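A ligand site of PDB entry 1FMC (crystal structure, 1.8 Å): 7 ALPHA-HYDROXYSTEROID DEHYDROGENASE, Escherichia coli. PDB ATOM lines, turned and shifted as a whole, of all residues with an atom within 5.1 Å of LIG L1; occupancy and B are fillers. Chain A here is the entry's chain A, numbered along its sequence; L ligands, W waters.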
ATOM      1  N   GLY A  97     -20.977  -1.714  30.794  1.00  0.00           N
ATOM      2  CA  GLY A  97     -20.187  -0.998  29.816  1.00  0.00           C
ATOM      3  C   GLY A  97     -19.493  -2.067  29.019  1.00  0.00           C
ATOM      4  O   GLY A  97     -19.927  -3.224  29.041  1.00  0.00           O
ATOM      5  N   GLY A  98     -18.417  -1.716  28.319  1.00  0.00           N
ATOM      6  CA  GLY A  98     -17.702  -2.709  27.545  1.00  0.00           C
ATOM      7  C   GLY A  98     -17.132  -2.172  26.257  1.00  0.00           C
ATOM      8  O   GLY A  98     -16.859  -0.984  26.136  1.00  0.00           O
ATOM      9  N   GLY A  99     -16.946  -3.050  25.276  1.00  0.00           N
ATOM     10  CA  GLY A  99     -16.378  -2.627  24.008  1.00  0.00           C
ATOM     11  C   GLY A  99     -15.174  -3.499  23.680  1.00  0.00           C
ATOM     12  O   GLY A  99     -15.228  -4.303  22.758  1.00  0.00           O
ATOM     13  N   GLY A 100     -14.099  -3.360  24.448  1.00  0.00           N
ATOM     14  CA  GLY A 100     -12.933  -4.168  24.193  1.00  0.00           C
ATOM     15  C   GLY A 100     -12.004  -3.714  23.067  1.00  0.00           C
ATOM     16  O   GLY A 100     -12.240  -2.715  22.384  1.00  0.00           O
ATOM     17  N   PRO A 101     -10.942  -4.488  22.832  1.00  0.00           N
ATOM     18  CA  PRO A 101      -9.919  -4.254  21.817  1.00  0.00           C
ATOM     19  C   PRO A 101     -10.512  -4.253  20.428  1.00  0.00           C
ATOM     20  O   PRO A 101     -11.361  -5.089  20.102  1.00  0.00           O
ATOM     21  CB  PRO A 101      -8.965  -5.435  21.981  1.00  0.00           C
ATOM     22  CG  PRO A 101      -9.332  -6.029  23.309  1.00  0.00           C
ATOM     23  CD  PRO A 101     -10.798  -5.835  23.407  1.00  0.00           C
ATOM     24  N   SER A 146     -12.205   2.314  33.781  1.00  0.00           N
ATOM     25  CA  SER A 146     -11.178   1.325  33.511  1.00  0.00           C
ATOM     26  C   SER A 146      -9.802   1.958  33.487  1.00  0.00           C
ATOM     27  O   SER A 146      -9.684   3.170  33.277  1.00  0.00           O
ATOM     28  CB  SER A 146     -11.441   0.630  32.156  1.00  0.00           C
ATOM     29  OG  SER A 146     -10.300  -0.076  31.699  1.00  0.00           O
ATOM     30  N   MET A 147      -8.766   1.160  33.717  1.00  0.00           N
ATOM     31  CA  MET A 147      -7.404   1.656  33.647  1.00  0.00           C
ATOM     32  C   MET A 147      -7.097   2.032  32.181  1.00  0.00           C
ATOM     33  O   MET A 147      -6.121   2.729  31.895  1.00  0.00           O
ATOM     34  CB  MET A 147      -6.407   0.595  34.126  1.00  0.00           C
ATOM     35  CG  MET A 147      -6.382   0.419  35.623  1.00  0.00           C
ATOM     36  SD  MET A 147      -5.037  -0.613  36.131  1.00  0.00           S
ATOM     37  CE  MET A 147      -3.628   0.548  36.082  1.00  0.00           C
ATOM     38  N   ALA A 148      -7.903   1.527  31.244  1.00  0.00           N
ATOM     39  CA  ALA A 148      -7.742   1.836  29.827  1.00  0.00           C
ATOM     40  C   ALA A 148      -7.831   3.360  29.612  1.00  0.00           C
ATOM     41  O   ALA A 148      -7.170   3.892  28.715  1.00  0.00           O
ATOM     42  CB  ALA A 148      -8.781   1.106  29.005  1.00  0.00           C
ATOM     43  N   ASN A 151      -4.172   4.073  30.306  1.00  0.00           N
ATOM     44  CA  ASN A 151      -3.194   3.298  29.559  1.00  0.00           C
ATOM     45  C   ASN A 151      -3.195   3.713  28.084  1.00  0.00           C
ATOM     46  O   ASN A 151      -4.188   4.286  27.587  1.00  0.00           O
ATOM     47  CB  ASN A 151      -3.522   1.819  29.621  1.00  0.00           C
ATOM     48  CG  ASN A 151      -3.391   1.276  30.946  1.00  0.00           C
ATOM     49  OD1 ASN A 151      -2.647   1.793  31.759  1.00  0.00           O
ATOM     50  ND2 ASN A 151      -4.123   0.201  31.216  1.00  0.00           N
ATOM     51  N   MET A 156      -6.776  -0.281  20.975  1.00  0.00           N
ATOM     52  CA  MET A 156      -7.585   0.184  22.091  1.00  0.00           C
ATOM     53  C   MET A 156      -8.263   1.538  21.862  1.00  0.00           C
ATOM     54  O   MET A 156      -8.846   2.086  22.795  1.00  0.00           O
ATOM     55  CB  MET A 156      -6.704   0.336  23.345  1.00  0.00           C
ATOM     56  CG  MET A 156      -6.204  -0.965  23.958  1.00  0.00           C
ATOM     57  SD  MET A 156      -7.541  -2.049  24.570  1.00  0.00           S
ATOM     58  CE  MET A 156      -8.562  -0.882  25.323  1.00  0.00           C
ATOM     59  N   TYR A 159     -12.272   1.641  23.001  1.00  0.00           N
ATOM     60  CA  TYR A 159     -12.427   1.320  24.414  1.00  0.00           C
ATOM     61  C   TYR A 159     -11.745   2.338  25.319  1.00  0.00           C
ATOM     62  O   TYR A 159     -12.394   2.937  26.175  1.00  0.00           O
ATOM     63  CB  TYR A 159     -11.877  -0.083  24.713  1.00  0.00           C
ATOM     64  CG  TYR A 159     -12.223  -0.578  26.116  1.00  0.00           C
ATOM     65  CD1 TYR A 159     -13.543  -0.852  26.485  1.00  0.00           C
ATOM     66  CD2 TYR A 159     -11.225  -0.737  27.091  1.00  0.00           C
ATOM     67  CE1 TYR A 159     -13.864  -1.283  27.776  1.00  0.00           C
ATOM     68  CE2 TYR A 159     -11.532  -1.159  28.376  1.00  0.00           C
ATOM     69  CZ  TYR A 159     -12.850  -1.427  28.705  1.00  0.00           C
ATOM     70  OH  TYR A 159     -13.169  -1.827  29.976  1.00  0.00           O
ATOM     71  N   PRO A 189     -10.859  -0.295  37.434  1.00  0.00           N
ATOM     72  CA  PRO A 189     -10.271  -1.606  37.730  1.00  0.00           C
ATOM     73  C   PRO A 189      -9.173  -1.978  36.737  1.00  0.00           C
ATOM     74  O   PRO A 189      -9.164  -1.496  35.594  1.00  0.00           O
ATOM     75  CB  PRO A 189     -11.459  -2.565  37.545  1.00  0.00           C
ATOM     76  CG  PRO A 189     -12.662  -1.705  37.565  1.00  0.00           C
ATOM     77  CD  PRO A 189     -12.210  -0.455  36.888  1.00  0.00           C
ATOM     78  N   GLY A 190      -8.236  -2.791  37.218  1.00  0.00           N
ATOM     79  CA  GLY A 190      -7.177  -3.315  36.387  1.00  0.00           C
ATOM     80  C   GLY A 190      -7.758  -4.653  35.935  1.00  0.00           C
ATOM     81  O   GLY A 190      -8.986  -4.768  35.795  1.00  0.00           O
ATOM     82  N   ALA A 191      -6.921  -5.661  35.749  1.00  0.00           N
ATOM     83  CA  ALA A 191      -7.407  -6.980  35.297  1.00  0.00           C
ATOM     84  C   ALA A 191      -8.247  -7.663  36.379  1.00  0.00           C
ATOM     85  O   ALA A 191      -7.724  -8.032  37.429  1.00  0.00           O
ATOM     86  CB  ALA A 191      -6.246  -7.874  34.900  1.00  0.00           C
ATOM     87  N   ALA A 196     -15.616 -11.671  31.080  1.00  0.00           N
ATOM     88  CA  ALA A 196     -15.126 -10.659  30.141  1.00  0.00           C
ATOM     89  C   ALA A 196     -13.596 -10.722  30.006  1.00  0.00           C
ATOM     90  O   ALA A 196     -13.080 -10.771  28.892  1.00  0.00           O
ATOM     91  CB  ALA A 196     -15.566  -9.278  30.588  1.00  0.00           C
ATOM     92  N   LEU A 197     -12.881 -10.734  31.128  1.00  0.00           N
ATOM     93  CA  LEU A 197     -11.421 -10.811  31.064  1.00  0.00           C
ATOM     94  C   LEU A 197     -11.037 -12.142  30.455  1.00  0.00           C
ATOM     95  O   LEU A 197     -10.141 -12.220  29.624  1.00  0.00           O
ATOM     96  CB  LEU A 197     -10.787 -10.689  32.454  1.00  0.00           C
ATOM     97  CG  LEU A 197      -9.252 -10.823  32.499  1.00  0.00           C
ATOM     98  CD1 LEU A 197      -8.605  -9.675  31.734  1.00  0.00           C
ATOM     99  CD2 LEU A 197      -8.767 -10.826  33.915  1.00  0.00           C
ATOM    100  N   SER A 199     -12.433 -13.818  28.220  1.00  0.00           N
ATOM    101  CA  SER A 199     -12.671 -13.899  26.785  1.00  0.00           C
ATOM    102  C   SER A 199     -11.512 -13.340  25.940  1.00  0.00           C
ATOM    103  O   SER A 199     -11.459 -13.563  24.732  1.00  0.00           O
ATOM    104  CB  SER A 199     -13.965 -13.168  26.426  1.00  0.00           C
ATOM    105  OG  SER A 199     -13.811 -11.779  26.617  1.00  0.00           O
ATOM    106  N   VAL A 200     -10.596 -12.612  26.570  1.00  0.00           N
ATOM    107  CA  VAL A 200      -9.488 -12.024  25.837  1.00  0.00           C
ATOM    108  C   VAL A 200      -8.109 -12.350  26.445  1.00  0.00           C
ATOM    109  O   VAL A 200      -7.060 -12.093  25.844  1.00  0.00           O
ATOM    110  CB  VAL A 200      -9.696 -10.480  25.688  1.00  0.00           C
ATOM    111  CG1 VAL A 200      -9.446  -9.763  27.006  1.00  0.00           C
ATOM    112  CG2 VAL A 200      -8.830  -9.916  24.585  1.00  0.00           C
ATOM    113  N   MET A 209       0.923  -9.959  32.775  1.00  0.00           N
ATOM    114  CA  MET A 209       0.151  -9.108  33.658  1.00  0.00           C
ATOM    115  C   MET A 209       0.698  -9.223  35.082  1.00  0.00           C
ATOM    116  O   MET A 209       1.066  -8.222  35.695  1.00  0.00           O
ATOM    117  CB  MET A 209      -1.325  -9.511  33.627  1.00  0.00           C
ATOM    118  CG  MET A 209      -1.982  -9.325  32.279  1.00  0.00           C
ATOM    119  SD  MET A 209      -3.739  -9.677  32.292  1.00  0.00           S
ATOM    120  CE  MET A 209      -4.365  -8.478  31.067  1.00  0.00           C
ATOM    121  N   GLN A 252      -2.005  -4.093  33.906  1.00  0.00           N
ATOM    122  CA  GLN A 252      -2.277  -5.329  33.204  1.00  0.00           C
ATOM    123  C   GLN A 252      -2.820  -4.971  31.811  1.00  0.00           C
ATOM    124  O   GLN A 252      -3.894  -4.344  31.682  1.00  0.00           O
ATOM    125  CB  GLN A 252      -3.284  -6.197  33.993  1.00  0.00           C
ATOM    126  CG  GLN A 252      -2.903  -6.481  35.478  1.00  0.00           C
ATOM    127  CD  GLN A 252      -3.267  -5.325  36.423  1.00  0.00           C
ATOM    128  OE1 GLN A 252      -4.329  -4.722  36.286  1.00  0.00           O
ATOM    129  NE2 GLN A 252      -2.380  -5.018  37.359  1.00  0.00           N
ATOM    130  N   GLU A 253      -2.052  -5.301  30.796  1.00  0.00           N
ATOM    131  CA  GLU A 253      -2.441  -4.990  29.418  1.00  0.00           C
ATOM    132  C   GLU A 253      -2.336  -6.227  28.577  1.00  0.00           C
ATOM    133  O   GLU A 253      -1.732  -7.216  29.003  1.00  0.00           O
ATOM    134  CB  GLU A 253      -1.548  -3.881  28.848  1.00  0.00           C
ATOM    135  CG  GLU A 253      -1.732  -2.544  29.543  1.00  0.00           C
ATOM    136  CD  GLU A 253      -0.948  -1.434  28.915  1.00  0.00           C
ATOM    137  OE1 GLU A 253       0.284  -1.391  29.082  1.00  0.00           O
ATOM    138  OE2 GLU A 253      -1.593  -0.589  28.252  1.00  0.00           O
ATOM    139  N   LEU A 254      -2.967  -6.166  27.400  1.00  0.00           N
ATOM    140  CA  LEU A 254      -2.990  -7.262  26.444  1.00  0.00           C
ATOM    141  C   LEU A 254      -1.722  -7.306  25.583  1.00  0.00           C
ATOM    142  O   LEU A 254      -1.424  -8.317  24.947  1.00  0.00           O
ATOM    143  CB  LEU A 254      -4.223  -7.151  25.556  1.00  0.00           C
ATOM    144  CG  LEU A 254      -5.564  -7.254  26.293  1.00  0.00           C
ATOM    145  CD1 LEU A 254      -6.705  -6.971  25.356  1.00  0.00           C
ATOM    146  CD2 LEU A 254      -5.680  -8.632  26.893  1.00  0.00           C
HETATM  147  C1  LIG L   1      -6.300  -4.826  29.486  1.00  0.00           C
HETATM  148  C2  LIG L   1      -6.108  -3.473  28.821  1.00  0.00           C
HETATM  149  C3  LIG L   1      -6.026  -2.340  29.845  1.00  0.00           C
HETATM  150  O1  LIG L   1      -5.874  -1.034  29.243  1.00  0.00           O
HETATM  151  C4  LIG L   1      -7.259  -2.345  30.756  1.00  0.00           C
HETATM  152  C5  LIG L   1      -7.534  -3.717  31.411  1.00  0.00           C
HETATM  153  C6  LIG L   1      -8.821  -3.639  32.217  1.00  0.00           C
HETATM  154  C7  LIG L   1     -10.038  -3.621  31.338  1.00  0.00           C
HETATM  155  O2  LIG L   1     -10.815  -2.643  31.251  1.00  0.00           O
HETATM  156  C8  LIG L   1     -10.148  -4.880  30.511  1.00  0.00           C
HETATM  157  C9  LIG L   1      -8.921  -4.914  29.561  1.00  0.00           C
HETATM  158  C10 LIG L   1      -7.554  -4.934  30.385  1.00  0.00           C
HETATM  159  C11 LIG L   1      -9.051  -6.032  28.548  1.00  0.00           C
HETATM  160  C12 LIG L   1     -10.411  -6.077  27.808  1.00  0.00           C
HETATM  161  C13 LIG L   1     -11.594  -6.143  28.756  1.00  0.00           C
HETATM  162  C14 LIG L   1     -11.458  -4.931  29.688  1.00  0.00           C
HETATM  163  C15 LIG L   1     -12.783  -4.916  30.409  1.00  0.00           C
HETATM  164  C16 LIG L   1     -13.762  -5.123  29.261  1.00  0.00           C
HETATM  165  C17 LIG L   1     -12.985  -5.823  28.123  1.00  0.00           C
HETATM  166  C18 LIG L   1     -11.647  -7.507  29.524  1.00  0.00           C
HETATM  167  C19 LIG L   1      -7.408  -6.283  31.091  1.00  0.00           C
HETATM  168  C20 LIG L   1     -13.832  -6.933  27.440  1.00  0.00           C
HETATM  169  C21 LIG L   1     -13.094  -7.647  26.291  1.00  0.00           C
HETATM  170  C22 LIG L   1     -15.123  -6.320  26.948  1.00  0.00           C
HETATM  171  C23 LIG L   1     -16.117  -7.319  26.417  1.00  0.00           C
HETATM  172  C24 LIG L   1     -17.342  -6.648  25.763  1.00  0.00           C
HETATM  173  O3  LIG L   1     -17.852  -5.676  26.320  1.00  0.00           O
HETATM  174  N1  LIG L   1     -17.771  -7.099  24.696  1.00  0.00           N
HETATM  175  P1  LG2 L   2     -19.234  -9.301  32.693  1.00  0.00           P
HETATM  176  O1  LG2 L   2     -19.407  -9.722  31.275  1.00  0.00           O
HETATM  177  O2  LG2 L   2     -18.686 -10.311  33.603  1.00  0.00           O
HETATM  178  O3  LG2 L   2     -20.651  -8.768  33.214  1.00  0.00           O
HETATM  179  C1  LG2 L   2     -21.320  -7.817  32.416  1.00  0.00           C
HETATM  180  C2  LG2 L   2     -22.765  -7.869  32.724  1.00  0.00           C
HETATM  181  O4  LG2 L   2     -23.305  -6.742  32.014  1.00  0.00           O
HETATM  182  C3  LG2 L   2     -23.457  -9.134  32.187  1.00  0.00           C
HETATM  183  O5  LG2 L   2     -24.362  -9.710  33.172  1.00  0.00           O
HETATM  184  C4  LG2 L   2     -24.219  -8.630  30.960  1.00  0.00           C
HETATM  185  O6  LG2 L   2     -25.392  -9.415  30.639  1.00  0.00           O
HETATM  186  C5  LG2 L   2     -24.500  -7.174  31.352  1.00  0.00           C
HETATM  187  N1  LG2 L   2     -24.736  -6.264  30.222  1.00  0.00           N
HETATM  188  C6  LG2 L   2     -24.012  -6.201  29.084  1.00  0.00           C
HETATM  189  N2  LG2 L   2     -24.497  -5.301  28.228  1.00  0.00           N
HETATM  190  C7  LG2 L   2     -25.539  -4.807  28.876  1.00  0.00           C
HETATM  191  C8  LG2 L   2     -26.387  -3.830  28.365  1.00  0.00           C
HETATM  192  N3  LG2 L   2     -26.216  -3.372  27.128  1.00  0.00           N
HETATM  193  N4  LG2 L   2     -27.413  -3.433  29.162  1.00  0.00           N
HETATM  194  C9  LG2 L   2     -27.571  -3.991  30.373  1.00  0.00           C
HETATM  195  N5  LG2 L   2     -26.754  -4.938  30.847  1.00  0.00           N
HETATM  196  C10 LG2 L   2     -25.724  -5.380  30.120  1.00  0.00           C
HETATM  197  O7  LG2 L   2     -18.412  -7.914  32.766  1.00  0.00           O
HETATM  198  P2  LG2 L   2     -17.493  -7.194  33.848  1.00  0.00           P
HETATM  199  O8  LG2 L   2     -16.081  -7.620  33.639  1.00  0.00           O
HETATM  200  O9  LG2 L   2     -18.058  -7.354  35.209  1.00  0.00           O
HETATM  201  O10 LG2 L   2     -17.551  -5.645  33.474  1.00  0.00           O
HETATM  202  C11 LG2 L   2     -18.538  -4.750  33.941  1.00  0.00           C
HETATM  203  C12 LG2 L   2     -17.904  -3.392  33.811  1.00  0.00           C
HETATM  204  O11 LG2 L   2     -16.570  -3.379  34.361  1.00  0.00           O
HETATM  205  C13 LG2 L   2     -17.767  -2.878  32.352  1.00  0.00           C
HETATM  206  O12 LG2 L   2     -18.107  -1.472  32.292  1.00  0.00           O
HETATM  207  C14 LG2 L   2     -16.300  -3.087  32.031  1.00  0.00           C
HETATM  208  O13 LG2 L   2     -15.842  -2.255  30.973  1.00  0.00           O
HETATM  209  C15 LG2 L   2     -15.695  -2.771  33.385  1.00  0.00           C
HETATM  210  N6  LG2 L   2     -14.321  -3.277  33.617  1.00  0.00           N
HETATM  211  C16 LG2 L   2     -14.034  -4.654  33.637  1.00  0.00           C
HETATM  212  C17 LG2 L   2     -12.730  -5.094  33.918  1.00  0.00           C
HETATM  213  C18 LG2 L   2     -12.306  -6.579  33.818  1.00  0.00           C
HETATM  214  O14 LG2 L   2     -11.113  -6.886  33.754  1.00  0.00           O
HETATM  215  N7  LG2 L   2     -13.262  -7.506  33.788  1.00  0.00           N
HETATM  216  C19 LG2 L   2     -11.741  -4.149  34.187  1.00  0.00           C
HETATM  217  C20 LG2 L   2     -12.039  -2.773  34.154  1.00  0.00           C
HETATM  218  C21 LG2 L   2     -13.323  -2.337  33.864  1.00  0.00           C
HETATM  219  O   HOH W   1     -14.649  -7.901  23.302  1.00  0.00           O
HETATM  220  O   HOH W   2      -4.204  -0.793  27.155  1.00  0.00           O
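The side-chain hydroxyl (OG) of Ser 146 lies within hydrogen-bond range of an oxygen (O2) of LIG L1 (2.7 Å).
The backbone NH of Gly 97 is in hydrogen-bond range of an oxygen (O12) of LG2 L2 (3.2 Å).
OH of Tyr 159 lies within hydrogen-bond range of O13 of LG2 L2 (2.9 Å).
An oxygen (O3) of LIG L1 sits at hydrogen-bond distance from the backbone NH of Gly 99 (3.0 Å).
The side-chain amide nitrogen (ND2) of Asn 151 sits at hydrogen-bond distance from an oxygen (O1) of LIG L1.
An oxygen (O2) of LIG L1 sits at hydrogen-bond distance from the side-chain hydroxyl (OH) of Tyr 159, 2.8 Å away.
Water W2 bridges O1 of LIG L1 (2.7 Å) and OE2 of Glu 253 (2.8 Å).
OE1 of Gln 252 lies within hydrogen-bond range of N of Ala 191, 2.8 Å away.
The side-chain hydroxyl (OG) of Ser 199 lies within hydrogen-bond range of the backbone carbonyl oxygen (O) of Ala 196, at 2.6 Å.
The backbone NH (N) of Ala 148 is in hydrogen-bond range of the side-chain hydroxyl (OG) of Ser 146, 2.9 Å away.
ND2 of Asn 151 lies close to O of Met 147, 3.3 Å away.
Residues that only touch LIG L1: Gly 98 (3.2 Å), Ala 148 (3.5 Å), Gly 190 (3.8 Å), Ala 196 (3.6 Å), Leu 197 (3.7 Å), Val 200 (3.9 Å), Met 209 (3.8 Å), Gln 252 (3.3 Å) and Glu 253 (3.9 Å).
Hydrophobic or aromatic side chains that line LIG L1: Ala 148, Tyr 159, Leu 197, Val 200 and Met 209.
13 residues have an atom within 4 Å of LIG L1: Gly 98, Gly 99, Ser 146, Ala 148, Asn 151, Tyr 159, Gly 190, Ala 196, Leu 197, Val 200, Met 209, Gln 252 and Glu 253.
The nearest printed residue that does not touch LIG L1 is Gly 100 (4.01 Å).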
